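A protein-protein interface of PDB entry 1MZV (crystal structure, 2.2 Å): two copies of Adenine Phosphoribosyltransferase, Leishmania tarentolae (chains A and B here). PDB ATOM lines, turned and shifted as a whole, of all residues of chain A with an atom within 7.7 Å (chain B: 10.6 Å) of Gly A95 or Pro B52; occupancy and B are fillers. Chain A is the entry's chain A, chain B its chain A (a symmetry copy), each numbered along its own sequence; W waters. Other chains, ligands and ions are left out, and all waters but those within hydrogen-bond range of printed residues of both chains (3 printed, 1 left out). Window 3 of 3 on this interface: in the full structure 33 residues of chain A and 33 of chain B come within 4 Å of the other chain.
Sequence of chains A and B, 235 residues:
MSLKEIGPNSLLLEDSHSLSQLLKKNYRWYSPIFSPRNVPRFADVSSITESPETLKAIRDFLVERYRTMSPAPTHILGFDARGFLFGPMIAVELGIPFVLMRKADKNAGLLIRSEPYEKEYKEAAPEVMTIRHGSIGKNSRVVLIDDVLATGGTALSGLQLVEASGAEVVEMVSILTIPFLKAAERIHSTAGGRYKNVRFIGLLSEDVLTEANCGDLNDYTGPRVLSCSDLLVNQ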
ATOM      1  N   ARG A  67       2.090  38.287  11.619  1.00  0.00           N
ATOM      2  CA  ARG A  67       3.363  38.307  10.903  1.00  0.00           C
ATOM      3  C   ARG A  67       4.533  38.634  11.828  1.00  0.00           C
ATOM      4  O   ARG A  67       5.595  38.018  11.720  1.00  0.00           O
ATOM      5  CB  ARG A  67       3.353  39.294   9.737  1.00  0.00           C
ATOM      6  CG  ARG A  67       3.077  38.639   8.395  1.00  0.00           C
ATOM      7  CD  ARG A  67       2.967  39.626   7.233  1.00  0.00           C
ATOM      8  NE  ARG A  67       2.284  39.058   6.070  1.00  0.00           N
ATOM      9  CZ  ARG A  67       1.789  39.776   5.059  1.00  0.00           C
ATOM     10  NH1 ARG A  67       1.879  41.103   5.060  1.00  0.00           N
ATOM     11  NH2 ARG A  67       1.185  39.169   4.043  1.00  0.00           N
ATOM     12  N   PRO A  73       1.806  31.924  14.576  1.00  0.00           N
ATOM     13  CA  PRO A  73       0.695  30.972  14.501  1.00  0.00           C
ATOM     14  C   PRO A  73       0.836  30.041  13.298  1.00  0.00           C
ATOM     15  O   PRO A  73       1.332  30.447  12.245  1.00  0.00           O
ATOM     16  CB  PRO A  73      -0.522  31.879  14.294  1.00  0.00           C
ATOM     17  CG  PRO A  73      -0.100  33.193  14.816  1.00  0.00           C
ATOM     18  CD  PRO A  73       1.339  33.319  14.527  1.00  0.00           C
ATOM     19  N   THR A  74       0.418  28.802  13.458  1.00  0.00           N
ATOM     20  CA  THR A  74       0.436  27.846  12.362  1.00  0.00           C
ATOM     21  C   THR A  74      -0.959  27.639  11.752  1.00  0.00           C
ATOM     22  O   THR A  74      -1.072  27.111  10.664  1.00  0.00           O
ATOM     23  CB  THR A  74       0.948  26.498  12.866  1.00  0.00           C
ATOM     24  OG1 THR A  74       0.060  26.003  13.871  1.00  0.00           O
ATOM     25  CG2 THR A  74       2.325  26.626  13.583  1.00  0.00           C
ATOM     26  N   ILE A  90      -7.335  36.568   6.854  1.00  0.00           N
ATOM     27  CA  ILE A  90      -6.060  36.650   7.597  1.00  0.00           C
ATOM     28  C   ILE A  90      -5.161  35.519   7.123  1.00  0.00           C
ATOM     29  O   ILE A  90      -3.996  35.740   6.838  1.00  0.00           O
ATOM     30  CB  ILE A  90      -6.169  36.542   9.152  1.00  0.00           C
ATOM     31  CG1 ILE A  90      -7.273  37.390   9.770  1.00  0.00           C
ATOM     32  CG2 ILE A  90      -4.858  36.903   9.793  1.00  0.00           C
ATOM     33  CD1 ILE A  90      -7.437  38.622   9.076  1.00  0.00           C
ATOM     34  N   ALA A  91      -5.723  34.306   7.079  1.00  0.00           N
ATOM     35  CA  ALA A  91      -4.968  33.084   6.834  1.00  0.00           C
ATOM     36  C   ALA A  91      -4.324  33.109   5.445  1.00  0.00           C
ATOM     37  O   ALA A  91      -3.197  32.654   5.263  1.00  0.00           O
ATOM     38  CB  ALA A  91      -5.861  31.877   6.985  1.00  0.00           C
ATOM     39  N   VAL A  92      -5.050  33.659   4.473  1.00  0.00           N
ATOM     40  CA  VAL A  92      -4.572  33.733   3.114  1.00  0.00           C
ATOM     41  C   VAL A  92      -3.316  34.597   3.010  1.00  0.00           C
ATOM     42  O   VAL A  92      -2.437  34.274   2.241  1.00  0.00           O
ATOM     43  CB  VAL A  92      -5.702  34.191   2.125  1.00  0.00           C
ATOM     44  CG1 VAL A  92      -6.034  35.680   2.248  1.00  0.00           C
ATOM     45  CG2 VAL A  92      -5.315  33.834   0.698  1.00  0.00           C
ATOM     46  N   GLU A  93      -3.212  35.649   3.812  1.00  0.00           N
ATOM     47  CA  GLU A  93      -1.999  36.457   3.832  1.00  0.00           C
ATOM     48  C   GLU A  93      -0.810  35.813   4.582  1.00  0.00           C
ATOM     49  O   GLU A  93       0.332  36.071   4.232  1.00  0.00           O
ATOM     50  CB  GLU A  93      -2.273  37.856   4.414  1.00  0.00           C
ATOM     51  CG  GLU A  93      -3.325  38.667   3.680  1.00  0.00           C
ATOM     52  CD  GLU A  93      -2.917  39.059   2.269  1.00  0.00           C
ATOM     53  OE1 GLU A  93      -1.760  39.337   2.032  1.00  0.00           O
ATOM     54  OE2 GLU A  93      -3.771  39.113   1.387  1.00  0.00           O
ATOM     55  N   LEU A  94      -1.094  34.990   5.597  1.00  0.00           N
ATOM     56  CA  LEU A  94      -0.071  34.350   6.423  1.00  0.00           C
ATOM     57  C   LEU A  94       0.437  33.027   5.850  1.00  0.00           C
ATOM     58  O   LEU A  94       1.481  32.497   6.293  1.00  0.00           O
ATOM     59  CB  LEU A  94      -0.624  34.077   7.824  1.00  0.00           C
ATOM     60  CG  LEU A  94      -1.121  35.256   8.657  1.00  0.00           C
ATOM     61  CD1 LEU A  94      -1.759  34.777   9.915  1.00  0.00           C
ATOM     62  CD2 LEU A  94       0.011  36.189   8.991  1.00  0.00           C
ATOM     63  N   GLY A  95      -0.282  32.484   4.875  1.00  0.00           N
ATOM     64  CA  GLY A  95       0.089  31.205   4.283  1.00  0.00           C
ATOM     65  C   GLY A  95      -0.131  30.047   5.237  1.00  0.00           C
ATOM     66  O   GLY A  95       0.631  29.090   5.217  1.00  0.00           O
ATOM     67  N   ILE A  96      -1.187  30.122   6.052  1.00  0.00           N
ATOM     68  CA  ILE A  96      -1.536  29.046   6.985  1.00  0.00           C
ATOM     69  C   ILE A  96      -2.990  28.577   6.831  1.00  0.00           C
ATOM     70  O   ILE A  96      -3.855  29.336   6.386  1.00  0.00           O
ATOM     71  CB  ILE A  96      -1.245  29.490   8.461  1.00  0.00           C
ATOM     72  CG1 ILE A  96      -2.140  30.668   8.869  1.00  0.00           C
ATOM     73  CG2 ILE A  96       0.248  29.813   8.614  1.00  0.00           C
ATOM     74  CD1 ILE A  96      -1.969  31.108  10.343  1.00  0.00           C
ATOM     75  N   PRO A  97      -3.263  27.336   7.230  1.00  0.00           N
ATOM     76  CA  PRO A  97      -4.621  26.797   7.165  1.00  0.00           C
ATOM     77  C   PRO A  97      -5.665  27.573   7.966  1.00  0.00           C
ATOM     78  O   PRO A  97      -5.408  28.051   9.080  1.00  0.00           O
ATOM     79  CB  PRO A  97      -4.478  25.366   7.738  1.00  0.00           C
ATOM     80  CG  PRO A  97      -3.035  25.053   7.636  1.00  0.00           C
ATOM     81  CD  PRO A  97      -2.306  26.342   7.763  1.00  0.00           C
ATOM     82  N   PHE A  98      -6.844  27.707   7.358  1.00  0.00           N
ATOM     83  CA  PHE A  98      -8.040  28.088   8.081  1.00  0.00           C
ATOM     84  C   PHE A  98      -8.895  26.873   8.320  1.00  0.00           C
ATOM     85  O   PHE A  98      -9.350  26.200   7.364  1.00  0.00           O
ATOM     86  CB  PHE A  98      -8.842  29.144   7.360  1.00  0.00           C
ATOM     87  CG  PHE A  98     -10.065  29.545   8.104  1.00  0.00           C
ATOM     88  CD1 PHE A  98      -9.970  30.325   9.241  1.00  0.00           C
ATOM     89  CD2 PHE A  98     -11.313  29.085   7.719  1.00  0.00           C
ATOM     90  CE1 PHE A  98     -11.095  30.663   9.947  1.00  0.00           C
ATOM     91  CE2 PHE A  98     -12.451  29.447   8.442  1.00  0.00           C
ATOM     92  CZ  PHE A  98     -12.342  30.212   9.534  1.00  0.00           C
ATOM     93  N   LEU B  19      -4.760  27.009 -10.726  1.00  0.00           N
ATOM     94  CA  LEU B  19      -5.876  26.942  -9.745  1.00  0.00           C
ATOM     95  C   LEU B  19      -6.728  25.709  -9.979  1.00  0.00           C
ATOM     96  O   LEU B  19      -7.182  25.089  -9.028  1.00  0.00           O
ATOM     97  CB  LEU B  19      -6.818  28.145  -9.875  1.00  0.00           C
ATOM     98  CG  LEU B  19      -7.620  28.715  -8.714  1.00  0.00           C
ATOM     99  CD1 LEU B  19      -8.820  29.335  -9.227  1.00  0.00           C
ATOM    100  CD2 LEU B  19      -7.903  27.758  -7.537  1.00  0.00           C
ATOM    101  N   LEU B  22      -4.681  22.893  -8.649  1.00  0.00           N
ATOM    102  CA  LEU B  22      -4.694  22.942  -7.178  1.00  0.00           C
ATOM    103  C   LEU B  22      -5.979  22.372  -6.615  1.00  0.00           C
ATOM    104  O   LEU B  22      -5.941  21.627  -5.650  1.00  0.00           O
ATOM    105  CB  LEU B  22      -4.459  24.354  -6.640  1.00  0.00           C
ATOM    106  CG  LEU B  22      -2.993  24.762  -6.764  1.00  0.00           C
ATOM    107  CD1 LEU B  22      -2.823  26.240  -6.548  1.00  0.00           C
ATOM    108  CD2 LEU B  22      -2.094  23.977  -5.815  1.00  0.00           C
ATOM    109  N   LEU B  23      -7.106  22.687  -7.250  1.00  0.00           N
ATOM    110  CA  LEU B  23      -8.408  22.296  -6.726  1.00  0.00           C
ATOM    111  C   LEU B  23      -8.645  20.817  -6.928  1.00  0.00           C
ATOM    112  O   LEU B  23      -9.176  20.145  -6.060  1.00  0.00           O
ATOM    113  CB  LEU B  23      -9.525  23.070  -7.411  1.00  0.00           C
ATOM    114  CG  LEU B  23      -9.682  24.513  -6.954  1.00  0.00           C
ATOM    115  CD1 LEU B  23     -10.605  25.205  -7.912  1.00  0.00           C
ATOM    116  CD2 LEU B  23     -10.237  24.622  -5.515  1.00  0.00           C
ATOM    117  N   ASN B  26      -6.375  19.140  -4.266  1.00  0.00           N
ATOM    118  CA  ASN B  26      -6.625  19.351  -2.846  1.00  0.00           C
ATOM    119  C   ASN B  26      -8.046  19.094  -2.401  1.00  0.00           C
ATOM    120  O   ASN B  26      -8.251  18.832  -1.239  1.00  0.00           O
ATOM    121  CB  ASN B  26      -6.180  20.762  -2.441  1.00  0.00           C
ATOM    122  CG  ASN B  26      -4.673  20.931  -2.549  1.00  0.00           C
ATOM    123  OD1 ASN B  26      -3.932  20.220  -1.892  1.00  0.00           O
ATOM    124  ND2 ASN B  26      -4.222  21.850  -3.386  1.00  0.00           N
ATOM    125  N   VAL B  45     -15.430  21.791   2.219  1.00  0.00           N
ATOM    126  CA  VAL B  45     -14.850  23.105   1.932  1.00  0.00           C
ATOM    127  C   VAL B  45     -13.565  23.341   2.708  1.00  0.00           C
ATOM    128  O   VAL B  45     -12.713  24.137   2.294  1.00  0.00           O
ATOM    129  CB  VAL B  45     -15.847  24.230   2.222  1.00  0.00           C
ATOM    130  CG1 VAL B  45     -15.929  24.512   3.742  1.00  0.00           C
ATOM    131  CG2 VAL B  45     -15.491  25.446   1.431  1.00  0.00           C
ATOM    132  N   SER B  46     -13.409  22.645   3.832  1.00  0.00           N
ATOM    133  CA  SER B  46     -12.210  22.801   4.640  1.00  0.00           C
ATOM    134  C   SER B  46     -10.981  22.233   3.941  1.00  0.00           C
ATOM    135  O   SER B  46      -9.874  22.648   4.232  1.00  0.00           O
ATOM    136  CB  SER B  46     -12.390  22.180   6.025  1.00  0.00           C
ATOM    137  OG  SER B  46     -12.300  20.774   5.969  1.00  0.00           O
ATOM    138  N   SER B  47     -11.179  21.322   2.993  1.00  0.00           N
ATOM    139  CA  SER B  47     -10.074  20.816   2.166  1.00  0.00           C
ATOM    140  C   SER B  47      -9.457  21.932   1.322  1.00  0.00           C
ATOM    141  O   SER B  47      -8.272  21.872   0.937  1.00  0.00           O
ATOM    142  CB  SER B  47     -10.547  19.643   1.294  1.00  0.00           C
ATOM    143  OG  SER B  47     -11.427  20.084   0.265  1.00  0.00           O
ATOM    144  N   ILE B  48     -10.259  22.963   1.046  1.00  0.00           N
ATOM    145  CA  ILE B  48      -9.779  24.165   0.357  1.00  0.00           C
ATOM    146  C   ILE B  48      -9.244  25.233   1.338  1.00  0.00           C
ATOM    147  O   ILE B  48      -8.153  25.746   1.172  1.00  0.00           O
ATOM    148  CB  ILE B  48     -10.905  24.732  -0.546  1.00  0.00           C
ATOM    149  CG1 ILE B  48     -11.445  23.644  -1.474  1.00  0.00           C
ATOM    150  CG2 ILE B  48     -10.418  25.907  -1.361  1.00  0.00           C
ATOM    151  CD1 ILE B  48     -10.393  22.875  -2.218  1.00  0.00           C
ATOM    152  N   THR B  49      -9.986  25.542   2.388  1.00  0.00           N
ATOM    153  CA  THR B  49      -9.504  26.564   3.331  1.00  0.00           C
ATOM    154  C   THR B  49      -8.260  26.152   4.119  1.00  0.00           C
ATOM    155  O   THR B  49      -7.543  27.023   4.612  1.00  0.00           O
ATOM    156  CB  THR B  49     -10.610  27.032   4.288  1.00  0.00           C
ATOM    157  OG1 THR B  49     -11.023  25.971   5.166  1.00  0.00           O
ATOM    158  CG2 THR B  49     -11.869  27.434   3.493  1.00  0.00           C
ATOM    159  N   GLU B  50      -8.012  24.843   4.240  1.00  0.00           N
ATOM    160  CA  GLU B  50      -6.824  24.323   4.937  1.00  0.00           C
ATOM    161  C   GLU B  50      -5.583  24.245   4.055  1.00  0.00           C
ATOM    162  O   GLU B  50      -4.480  23.997   4.554  1.00  0.00           O
ATOM    163  CB  GLU B  50      -7.100  22.960   5.561  1.00  0.00           C
ATOM    164  CG  GLU B  50      -8.165  23.032   6.641  1.00  0.00           C
ATOM    165  CD  GLU B  50      -8.477  21.688   7.257  1.00  0.00           C
ATOM    166  OE1 GLU B  50      -7.625  20.787   7.117  1.00  0.00           O
ATOM    167  OE2 GLU B  50      -9.554  21.552   7.911  1.00  0.00           O
ATOM    168  N   SER B  51      -5.766  24.482   2.762  1.00  0.00           N
ATOM    169  CA  SER B  51      -4.683  24.530   1.788  1.00  0.00           C
ATOM    170  C   SER B  51      -4.377  25.997   1.451  1.00  0.00           C
ATOM    171  O   SER B  51      -5.040  26.599   0.608  1.00  0.00           O
ATOM    172  CB  SER B  51      -5.106  23.778   0.514  1.00  0.00           C
ATOM    173  OG  SER B  51      -4.108  23.866  -0.496  1.00  0.00           O
ATOM    174  N   PRO B  52      -3.377  26.584   2.102  1.00  0.00           N
ATOM    175  CA  PRO B  52      -3.070  28.007   1.866  1.00  0.00           C
ATOM    176  C   PRO B  52      -2.819  28.343   0.386  1.00  0.00           C
ATOM    177  O   PRO B  52      -3.229  29.397  -0.093  1.00  0.00           O
ATOM    178  CB  PRO B  52      -1.815  28.258   2.706  1.00  0.00           C
ATOM    179  CG  PRO B  52      -1.711  27.095   3.673  1.00  0.00           C
ATOM    180  CD  PRO B  52      -2.477  25.959   3.087  1.00  0.00           C
ATOM    181  N   GLU B  53      -2.182  27.429  -0.333  1.00  0.00           N
ATOM    182  CA  GLU B  53      -1.876  27.644  -1.742  1.00  0.00           C
ATOM    183  C   GLU B  53      -3.176  27.730  -2.568  1.00  0.00           C
ATOM    184  O   GLU B  53      -3.314  28.607  -3.411  1.00  0.00           O
ATOM    185  CB  GLU B  53      -0.925  26.543  -2.227  1.00  0.00           C
ATOM    186  CG  GLU B  53      -0.614  26.570  -3.703  1.00  0.00           C
ATOM    187  CD  GLU B  53       0.570  25.673  -4.073  1.00  0.00           C
ATOM    188  OE1 GLU B  53       1.233  25.955  -5.096  1.00  0.00           O
ATOM    189  OE2 GLU B  53       0.830  24.697  -3.331  1.00  0.00           O
ATOM    190  N   THR B  54      -4.132  26.859  -2.279  1.00  0.00           N
ATOM    191  CA  THR B  54      -5.388  26.834  -3.019  1.00  0.00           C
ATOM    192  C   THR B  54      -6.252  28.058  -2.692  1.00  0.00           C
ATOM    193  O   THR B  54      -6.746  28.743  -3.587  1.00  0.00           O
ATOM    194  CB  THR B  54      -6.160  25.557  -2.713  1.00  0.00           C
ATOM    195  OG1 THR B  54      -5.338  24.400  -2.968  1.00  0.00           O
ATOM    196  CG2 THR B  54      -7.346  25.412  -3.680  1.00  0.00           C
ATOM    197  N   LEU B  55      -6.433  28.321  -1.401  1.00  0.00           N
ATOM    198  CA  LEU B  55      -7.148  29.496  -0.964  1.00  0.00           C
ATOM    199  C   LEU B  55      -6.577  30.757  -1.609  1.00  0.00           C
ATOM    200  O   LEU B  55      -7.329  31.567  -2.113  1.00  0.00           O
ATOM    201  CB  LEU B  55      -7.140  29.602   0.554  1.00  0.00           C
ATOM    202  CG  LEU B  55      -8.168  30.557   1.164  1.00  0.00           C
ATOM    203  CD1 LEU B  55      -9.593  30.127   0.891  1.00  0.00           C
ATOM    204  CD2 LEU B  55      -7.956  30.660   2.669  1.00  0.00           C
ATOM    205  N   LYS B  56      -5.259  30.894  -1.638  1.00  0.00           N
ATOM    206  CA  LYS B  56      -4.627  32.079  -2.202  1.00  0.00           C
ATOM    207  C   LYS B  56      -4.862  32.166  -3.701  1.00  0.00           C
ATOM    208  O   LYS B  56      -5.164  33.238  -4.219  1.00  0.00           O
ATOM    209  CB  LYS B  56      -3.134  32.104  -1.883  1.00  0.00           C
ATOM    210  CG  LYS B  56      -2.396  33.317  -2.501  1.00  0.00           C
ATOM    211  CD  LYS B  56      -0.969  33.478  -2.008  1.00  0.00           C
ATOM    212  CE  LYS B  56      -0.345  34.796  -2.536  1.00  0.00           C
ATOM    213  NZ  LYS B  56      -0.422  35.047  -4.050  1.00  0.00           N
ATOM    214  N   ALA B  57      -4.756  31.033  -4.387  1.00  0.00           N
ATOM    215  CA  ALA B  57      -4.994  30.964  -5.830  1.00  0.00           C
ATOM    216  C   ALA B  57      -6.441  31.370  -6.181  1.00  0.00           C
ATOM    217  O   ALA B  57      -6.664  32.053  -7.166  1.00  0.00           O
ATOM    218  CB  ALA B  57      -4.674  29.568  -6.353  1.00  0.00           C
ATOM    219  N   ILE B  58      -7.403  30.995  -5.348  1.00  0.00           N
ATOM    220  CA  ILE B  58      -8.806  31.363  -5.587  1.00  0.00           C
ATOM    221  C   ILE B  58      -8.920  32.888  -5.465  1.00  0.00           C
ATOM    222  O   ILE B  58      -9.464  33.559  -6.328  1.00  0.00           O
ATOM    223  CB  ILE B  58      -9.755  30.675  -4.562  1.00  0.00           C
ATOM    224  CG1 ILE B  58      -9.895  29.193  -4.837  1.00  0.00           C
ATOM    225  CG2 ILE B  58     -11.132  31.371  -4.546  1.00  0.00           C
ATOM    226  CD1 ILE B  58     -10.512  28.437  -3.680  1.00  0.00           C
ATOM    227  N   ARG B  59      -8.383  33.398  -4.375  1.00  0.00           N
ATOM    228  CA  ARG B  59      -8.370  34.823  -4.075  1.00  0.00           C
ATOM    229  C   ARG B  59      -7.725  35.626  -5.212  1.00  0.00           C
ATOM    230  O   ARG B  59      -8.310  36.579  -5.727  1.00  0.00           O
ATOM    231  CB  ARG B  59      -7.629  35.044  -2.747  1.00  0.00           C
ATOM    232  CG  ARG B  59      -7.763  36.435  -2.139  1.00  0.00           C
ATOM    233  CD  ARG B  59      -6.874  37.530  -2.774  1.00  0.00           C
ATOM    234  NE  ARG B  59      -5.472  37.157  -2.869  1.00  0.00           N
ATOM    235  CZ  ARG B  59      -4.571  37.323  -1.894  1.00  0.00           C
ATOM    236  NH1 ARG B  59      -4.925  37.834  -0.714  1.00  0.00           N
ATOM    237  NH2 ARG B  59      -3.303  36.977  -2.088  1.00  0.00           N
ATOM    238  N   ASP B  60      -6.514  35.256  -5.579  1.00  0.00           N
ATOM    239  CA  ASP B  60      -5.821  35.945  -6.641  1.00  0.00           C
ATOM    240  C   ASP B  60      -6.618  35.879  -7.946  1.00  0.00           C
ATOM    241  O   ASP B  60      -6.753  36.880  -8.633  1.00  0.00           O
ATOM    242  CB  ASP B  60      -4.439  35.335  -6.880  1.00  0.00           C
ATOM    243  CG  ASP B  60      -3.498  35.613  -5.760  1.00  0.00           C
ATOM    244  OD1 ASP B  60      -2.453  34.941  -5.705  1.00  0.00           O
ATOM    245  OD2 ASP B  60      -3.712  36.488  -4.894  1.00  0.00           O
ATOM    246  N   PHE B  61      -7.135  34.707  -8.276  1.00  0.00           N
ATOM    247  CA  PHE B  61      -7.860  34.561  -9.517  1.00  0.00           C
ATOM    248  C   PHE B  61      -9.083  35.475  -9.572  1.00  0.00           C
ATOM    249  O   PHE B  61      -9.292  36.175 -10.574  1.00  0.00           O
ATOM    250  CB  PHE B  61      -8.318  33.123  -9.751  1.00  0.00           C
ATOM    251  CG  PHE B  61      -9.020  32.947 -11.060  1.00  0.00           C
ATOM    252  CD1 PHE B  61      -8.296  32.974 -12.245  1.00  0.00           C
ATOM    253  CD2 PHE B  61     -10.400  32.834 -11.125  1.00  0.00           C
ATOM    254  CE1 PHE B  61      -8.952  32.832 -13.477  1.00  0.00           C
ATOM    255  CE2 PHE B  61     -11.074  32.688 -12.355  1.00  0.00           C
ATOM    256  CZ  PHE B  61     -10.358  32.684 -13.512  1.00  0.00           C
ATOM    257  N   PHE B  86     -15.192  32.729   1.321  1.00  0.00           N
ATOM    258  CA  PHE B  86     -14.509  33.188   0.122  1.00  0.00           C
ATOM    259  C   PHE B  86     -14.750  34.648  -0.219  1.00  0.00           C
ATOM    260  O   PHE B  86     -13.875  35.302  -0.755  1.00  0.00           O
ATOM    261  CB  PHE B  86     -14.921  32.305  -1.054  1.00  0.00           C
ATOM    262  CG  PHE B  86     -14.549  30.883  -0.864  1.00  0.00           C
ATOM    263  CD1 PHE B  86     -13.221  30.488  -0.968  1.00  0.00           C
ATOM    264  CD2 PHE B  86     -15.500  29.945  -0.532  1.00  0.00           C
ATOM    265  CE1 PHE B  86     -12.856  29.180  -0.754  1.00  0.00           C
ATOM    266  CE2 PHE B  86     -15.132  28.638  -0.283  1.00  0.00           C
ATOM    267  CZ  PHE B  86     -13.798  28.256  -0.421  1.00  0.00           C
ATOM    268  N   MET B  89     -12.488  37.807   1.525  1.00  0.00           N
ATOM    269  CA  MET B  89     -11.120  37.940   1.020  1.00  0.00           C
ATOM    270  C   MET B  89     -11.059  38.522  -0.371  1.00  0.00           C
ATOM    271  O   MET B  89     -10.007  39.076  -0.743  1.00  0.00           O
ATOM    272  CB  MET B  89     -10.324  36.616   1.124  1.00  0.00           C
ATOM    273  CG  MET B  89     -10.508  35.636   0.046  1.00  0.00           C
ATOM    274  SD  MET B  89      -9.664  34.100   0.425  1.00  0.00           S
ATOM    275  CE  MET B  89     -10.282  33.205  -0.914  1.00  0.00           C
HETATM  276  O   HOH W   1      -5.459  28.813   4.017  1.00  0.00           O
HETATM  277  O   HOH W   2      -1.884  31.802   1.540  1.00  0.00           O
HETATM  278  O   HOH W   3      -0.996  37.626  -0.190  1.00  0.00           O
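Of chain B, only Pro B52 comes within 4 Å of Gly A95.
Pro B52 touches just these residues of chain A: Gly A95 (3.4 Å), Ile A96 (3.7 Å) and Pro A97 (3.9 Å).
Leu A94 touches none of the printed residues of chain B.
Of chain B, only Pro B52 (3.7 Å) comes within 4 Å of Ile A96.
Of the printed residues of chain B, Pro A97 touches Thr B49, Glu B50 and Pro B52.
Of the printed residues of chain A, Glu B50 touches Pro A97 (3.5 Å) and Phe A98 (3.5 Å).
Printed residues of chain B within 4 Å of Glu A93: Arg B59.
Printed residues of chain A within 4 Å of Lys B56: Val A92 (3.5 Å).
Of the printed residues of chain A, Arg B59 touches Val A92 (3.8 Å) and Glu A93 (2.7 Å).
Thr A74 touches none of the printed residues of chain B.
Phe B61 touches none of the printed residues of chain A.
The nearest residue of chain A that does not touch Pro B52 is Val A92 (5.0 Å).
The nearest printed residue of chain A that does not touch Thr B49 is Ile A96 (4.7 Å).
No position is printed for both chains.
Of the 10 pairs that touch across the chains among the printed residues, none has its exchanged pair printed and touching as well.
Among the printed residues, merely in contact across the chains: Val A92 with Lys B56 (3.5 Å), Val A92 with Arg B59 (3.8 Å), Gly A95 with Pro B52 (3.4 Å), Ile A96 with Pro B52 (3.7 Å), Pro A97 with Thr B49 (3.9 Å), Pro A97 with Glu B50 (3.5 Å), Pro A97 with Pro B52 (3.9 Å) and Phe A98 with Glu B50 (3.5 Å).
Of the 12 printed residues of chain A, 6 touch a printed residue of chain B.
Of the 23 printed residues of chain B, 5 touch a printed residue of chain A.
Among the printed residues, 10 pairs touch across the chains.
Among the printed residues, Asp or Glu carboxylates within 4 Å of a Lys or Arg side-chain nitrogen of the other chain: Glu A93 with Arg B59.
OE2 of Glu B50 is in hydrogen-bond range of OG of Ser B46 (3.5 Å).
NZ of Lys B56 lies within salt-bridge range of OD1 of Asp B60 (2.6 Å).
The guanidinium group (NH2) of Arg A67 lies within salt-bridge range of the side-chain carboxylate (OE1) of Glu A93, at 3.6 Å.
O of Ala A91 sits at hydrogen-bond distance from N of Ile A96 (3.3 Å).
NE of Arg B59 lies within salt-bridge range of OD2 of Asp B60, 2.8 Å away.
The guanidinium group of Arg B59 lies within salt-bridge range of the side-chain carboxylate of Glu A93 (2.7 Å).
The backbone carbonyl oxygen of Phe A98 is in hydrogen-bond range of the side-chain hydroxyl of Thr B49 (2.8 Å).
Water W2 bridges the backbone carbonyl oxygen (O) of Val A92 (2.6 Å) and the backbone carbonyl oxygen (O) of Pro B52 (3.2 Å).
Water W1 bridges O of Thr B49 and O of Ile A96.
Water W3 lies within hydrogen-bond range of OE1 of Glu A93 and NH2 of Arg B59.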
